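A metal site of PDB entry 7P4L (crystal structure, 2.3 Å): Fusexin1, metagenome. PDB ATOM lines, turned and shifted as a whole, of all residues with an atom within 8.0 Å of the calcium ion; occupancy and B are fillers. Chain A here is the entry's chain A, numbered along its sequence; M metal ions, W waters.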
ATOM      1  N   GLY A  89      13.918 -32.498  15.687  1.00  0.00           N
ATOM      2  CA  GLY A  89      14.528 -33.146  14.552  1.00  0.00           C
ATOM      3  C   GLY A  89      13.570 -33.700  13.528  1.00  0.00           C
ATOM      4  O   GLY A  89      14.022 -34.334  12.565  1.00  0.00           O
ATOM      5  N   PHE A  90      12.265 -33.517  13.713  1.00  0.00           N
ATOM      6  CA  PHE A  90      11.306 -33.994  12.723  1.00  0.00           C
ATOM      7  C   PHE A  90      11.414 -33.135  11.464  1.00  0.00           C
ATOM      8  O   PHE A  90      11.484 -31.901  11.548  1.00  0.00           O
ATOM      9  CB  PHE A  90       9.891 -33.949  13.287  1.00  0.00           C
ATOM     10  CG  PHE A  90       9.693 -34.857  14.479  1.00  0.00           C
ATOM     11  CD1 PHE A  90       9.470 -36.212  14.302  1.00  0.00           C
ATOM     12  CD2 PHE A  90       9.723 -34.352  15.772  1.00  0.00           C
ATOM     13  CE1 PHE A  90       9.293 -37.048  15.381  1.00  0.00           C
ATOM     14  CE2 PHE A  90       9.542 -35.194  16.858  1.00  0.00           C
ATOM     15  CZ  PHE A  90       9.320 -36.539  16.661  1.00  0.00           C
ATOM     16  N   ASP A  91      11.440 -33.782  10.302  1.00  0.00           N
ATOM     17  CA  ASP A  91      11.676 -33.065   9.047  1.00  0.00           C
ATOM     18  C   ASP A  91      10.438 -32.289   8.603  1.00  0.00           C
ATOM     19  O   ASP A  91      10.549 -31.121   8.216  1.00  0.00           O
ATOM     20  CB  ASP A  91      12.086 -34.050   7.956  1.00  0.00           C
ATOM     21  CG  ASP A  91      12.434 -33.348   6.643  1.00  0.00           C
ATOM     22  OD1 ASP A  91      12.678 -32.119   6.658  1.00  0.00           O
ATOM     23  OD2 ASP A  91      12.468 -34.035   5.596  1.00  0.00           O
ATOM     24  N   THR A  92       9.268 -32.912   8.667  1.00  0.00           N
ATOM     25  CA  THR A  92       8.042 -32.302   8.180  1.00  0.00           C
ATOM     26  C   THR A  92       6.978 -32.311   9.270  1.00  0.00           C
ATOM     27  O   THR A  92       7.061 -33.042  10.250  1.00  0.00           O
ATOM     28  CB  THR A  92       7.508 -33.036   6.935  1.00  0.00           C
ATOM     29  OG1 THR A  92       7.175 -34.383   7.284  1.00  0.00           O
ATOM     30  CG2 THR A  92       8.554 -33.038   5.839  1.00  0.00           C
ATOM     31  N   GLU A  93       5.966 -31.470   9.060  1.00  0.00           N
ATOM     32  CA  GLU A  93       4.842 -31.406   9.988  1.00  0.00           C
ATOM     33  C   GLU A  93       4.150 -32.754  10.103  1.00  0.00           C
ATOM     34  O   GLU A  93       3.745 -33.174  11.186  1.00  0.00           O
ATOM     35  CB  GLU A  93       3.863 -30.325   9.524  1.00  0.00           C
ATOM     36  CG  GLU A  93       2.618 -30.146  10.373  1.00  0.00           C
ATOM     37  CD  GLU A  93       1.755 -28.998   9.877  1.00  0.00           C
ATOM     38  OE1 GLU A  93       2.065 -28.444   8.804  1.00  0.00           O
ATOM     39  OE2 GLU A  93       0.777 -28.644  10.560  1.00  0.00           O
ATOM     40  N   ASP A  95       5.509 -35.672   9.759  1.00  0.00           N
ATOM     41  CA  ASP A  95       6.356 -36.532  10.597  1.00  0.00           C
ATOM     42  C   ASP A  95       6.066 -36.297  12.074  1.00  0.00           C
ATOM     43  O   ASP A  95       5.928 -37.244  12.857  1.00  0.00           O
ATOM     44  CB  ASP A  95       7.832 -36.268  10.296  1.00  0.00           C
ATOM     45  CG  ASP A  95       8.217 -36.668   8.885  1.00  0.00           C
ATOM     46  OD1 ASP A  95       7.503 -37.487   8.277  1.00  0.00           O
ATOM     47  OD2 ASP A  95       9.237 -36.145   8.391  1.00  0.00           O
ATOM     48  N   TYR A 120      10.268 -24.775  13.454  1.00  0.00           N
ATOM     49  CA  TYR A 120      11.373 -23.850  13.643  1.00  0.00           C
ATOM     50  C   TYR A 120      12.242 -23.822  12.391  1.00  0.00           C
ATOM     51  O   TYR A 120      12.386 -24.824  11.683  1.00  0.00           O
ATOM     52  CB  TYR A 120      12.220 -24.199  14.873  1.00  0.00           C
ATOM     53  CG  TYR A 120      12.790 -25.600  14.911  1.00  0.00           C
ATOM     54  CD1 TYR A 120      12.019 -26.672  15.320  1.00  0.00           C
ATOM     55  CD2 TYR A 120      14.114 -25.844  14.557  1.00  0.00           C
ATOM     56  CE1 TYR A 120      12.540 -27.956  15.367  1.00  0.00           C
ATOM     57  CE2 TYR A 120      14.639 -27.123  14.597  1.00  0.00           C
ATOM     58  CZ  TYR A 120      13.842 -28.171  14.995  1.00  0.00           C
ATOM     59  OH  TYR A 120      14.341 -29.448  15.049  1.00  0.00           O
ATOM     60  N   TYR A 121      12.825 -22.648  12.139  1.00  0.00           N
ATOM     61  CA  TYR A 121      13.637 -22.439  10.944  1.00  0.00           C
ATOM     62  C   TYR A 121      14.820 -23.399  10.946  1.00  0.00           C
ATOM     63  O   TYR A 121      15.522 -23.533  11.964  1.00  0.00           O
ATOM     64  CB  TYR A 121      14.107 -20.983  10.912  1.00  0.00           C
ATOM     65  CG  TYR A 121      14.797 -20.548   9.644  1.00  0.00           C
ATOM     66  CD1 TYR A 121      14.084 -20.371   8.468  1.00  0.00           C
ATOM     67  CD2 TYR A 121      16.170 -20.278   9.628  1.00  0.00           C
ATOM     68  CE1 TYR A 121      14.707 -19.957   7.299  1.00  0.00           C
ATOM     69  CE2 TYR A 121      16.805 -19.870   8.462  1.00  0.00           C
ATOM     70  CZ  TYR A 121      16.062 -19.710   7.311  1.00  0.00           C
ATOM     71  OH  TYR A 121      16.681 -19.303   6.149  1.00  0.00           O
ATOM     72  N   SER A 122      15.031 -24.072   9.819  1.00  0.00           N
ATOM     73  CA  SER A 122      16.094 -25.068   9.675  1.00  0.00           C
ATOM     74  C   SER A 122      16.856 -24.808   8.392  1.00  0.00           C
ATOM     75  O   SER A 122      16.296 -24.937   7.287  1.00  0.00           O
ATOM     76  CB  SER A 122      15.508 -26.486   9.697  1.00  0.00           C
ATOM     77  OG  SER A 122      16.510 -27.468   9.570  1.00  0.00           O
ATOM     78  N   VAL A 123      18.141 -24.444   8.501  1.00  0.00           N
ATOM     79  CA  VAL A 123      18.966 -24.278   7.308  1.00  0.00           C
ATOM     80  C   VAL A 123      19.279 -25.632   6.685  1.00  0.00           C
ATOM     81  O   VAL A 123      19.318 -25.767   5.452  1.00  0.00           O
ATOM     82  CB  VAL A 123      20.251 -23.498   7.630  1.00  0.00           C
ATOM     83  CG1 VAL A 123      19.919 -22.080   8.094  1.00  0.00           C
ATOM     84  CG2 VAL A 123      21.099 -24.224   8.679  1.00  0.00           C
ATOM     85  N   THR A 124      19.508 -26.651   7.517  1.00  0.00           N
ATOM     86  CA  THR A 124      19.941 -27.945   7.016  1.00  0.00           C
ATOM     87  C   THR A 124      18.795 -28.720   6.381  1.00  0.00           C
ATOM     88  O   THR A 124      18.996 -29.443   5.393  1.00  0.00           O
ATOM     89  CB  THR A 124      20.562 -28.761   8.153  1.00  0.00           C
ATOM     90  OG1 THR A 124      21.765 -28.114   8.602  1.00  0.00           O
ATOM     91  CG2 THR A 124      20.876 -30.179   7.692  1.00  0.00           C
ATOM     92  N   SER A 125      17.584 -28.585   6.914  1.00  0.00           N
ATOM     93  CA  SER A 125      16.393 -29.254   6.383  1.00  0.00           C
ATOM     94  C   SER A 125      15.316 -28.190   6.174  1.00  0.00           C
ATOM     95  O   SER A 125      14.311 -28.148   6.884  1.00  0.00           O
ATOM     96  CB  SER A 125      15.918 -30.351   7.337  1.00  0.00           C
ATOM     97  OG  SER A 125      14.843 -31.111   6.788  1.00  0.00           O
ATOM     98  N   PRO A 126      15.521 -27.313   5.203  1.00  0.00           N
ATOM     99  CA  PRO A 126      14.597 -26.191   5.020  1.00  0.00           C
ATOM    100  C   PRO A 126      13.261 -26.649   4.445  1.00  0.00           C
ATOM    101  O   PRO A 126      13.149 -27.713   3.831  1.00  0.00           O
ATOM    102  CB  PRO A 126      15.334 -25.267   4.054  1.00  0.00           C
ATOM    103  CG  PRO A 126      16.223 -26.172   3.278  1.00  0.00           C
ATOM    104  CD  PRO A 126      16.613 -27.287   4.215  1.00  0.00           C
ATOM    105  N   VAL A 127      12.230 -25.828   4.637  1.00  0.00           N
ATOM    106  CA  VAL A 127      12.324 -24.550   5.360  1.00  0.00           C
ATOM    107  C   VAL A 127      12.316 -24.742   6.886  1.00  0.00           C
ATOM    108  O   VAL A 127      12.943 -23.964   7.607  1.00  0.00           O
ATOM    109  CB  VAL A 127      11.195 -23.608   4.947  1.00  0.00           C
ATOM    110  CG1 VAL A 127      11.308 -22.282   5.677  1.00  0.00           C
ATOM    111  CG2 VAL A 127      11.207 -23.396   3.440  1.00  0.00           C
ATOM    112  N   TYR A 128      11.611 -25.768   7.358  1.00  0.00           N
ATOM    113  CA  TYR A 128      11.424 -25.971   8.795  1.00  0.00           C
ATOM    114  C   TYR A 128      11.736 -27.401   9.195  1.00  0.00           C
ATOM    115  O   TYR A 128      11.648 -28.329   8.378  1.00  0.00           O
ATOM    116  CB  TYR A 128       9.988 -25.651   9.214  1.00  0.00           C
ATOM    117  CG  TYR A 128       9.534 -24.248   8.890  1.00  0.00           C
ATOM    118  CD1 TYR A 128       9.879 -23.180   9.708  1.00  0.00           C
ATOM    119  CD2 TYR A 128       8.729 -23.998   7.790  1.00  0.00           C
ATOM    120  CE1 TYR A 128       9.464 -21.890   9.415  1.00  0.00           C
ATOM    121  CE2 TYR A 128       8.307 -22.711   7.491  1.00  0.00           C
ATOM    122  CZ  TYR A 128       8.675 -21.664   8.305  1.00  0.00           C
ATOM    123  OH  TYR A 128       8.254 -20.390   8.009  1.00  0.00           O
ATOM    124  N   ASP A 129      12.131 -27.552  10.456  1.00  0.00           N
ATOM    125  CA  ASP A 129      11.996 -28.784  11.220  1.00  0.00           C
ATOM    126  C   ASP A 129      10.956 -28.547  12.313  1.00  0.00           C
ATOM    127  O   ASP A 129      10.470 -27.431  12.492  1.00  0.00           O
ATOM    128  CB  ASP A 129      13.335 -29.229  11.812  1.00  0.00           C
ATOM    129  CG  ASP A 129      14.199 -29.981  10.803  1.00  0.00           C
ATOM    130  OD1 ASP A 129      13.750 -30.171   9.658  1.00  0.00           O
ATOM    131  OD2 ASP A 129      15.327 -30.378  11.163  1.00  0.00           O
ATOM    132  N   TYR A 130      10.624 -29.603  13.060  1.00  0.00           N
ATOM    133  CA  TYR A 130       9.489 -29.537  13.969  1.00  0.00           C
ATOM    134  C   TYR A 130       9.815 -30.170  15.320  1.00  0.00           C
ATOM    135  O   TYR A 130      10.487 -31.201  15.381  1.00  0.00           O
ATOM    136  CB  TYR A 130       8.269 -30.233  13.355  1.00  0.00           C
ATOM    137  CG  TYR A 130       7.734 -29.505  12.140  1.00  0.00           C
ATOM    138  CD1 TYR A 130       8.374 -29.618  10.905  1.00  0.00           C
ATOM    139  CD2 TYR A 130       6.632 -28.677  12.222  1.00  0.00           C
ATOM    140  CE1 TYR A 130       7.918 -28.956   9.798  1.00  0.00           C
ATOM    141  CE2 TYR A 130       6.157 -28.002  11.115  1.00  0.00           C
ATOM    142  CZ  TYR A 130       6.810 -28.143   9.908  1.00  0.00           C
ATOM    143  OH  TYR A 130       6.350 -27.478   8.788  1.00  0.00           O
HETATM  144 CA    CA M   1      12.809 -30.000   7.265  1.00  0.00          CA
HETATM  145  O   HOH W   1      11.342 -29.422   5.245  1.00  0.00           O
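The calcium ion is bound by OD1 of Asp 91 (2.2 Å), O of Tyr 128 (2.3 Å), OG of Ser 125 (2.4 Å), O of Ser 125 (2.4 Å), water W1 (2.6 Å), OD1 of Asp 129 (2.6 Å) and O of Asp 91 (2.7 Å).
N of Ser 125 is in hydrogen-bond range of OG of Ser 122 (3.1 Å).
O of Asp 129 lies within hydrogen-bond range of N of Tyr 120, 2.8 Å away.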
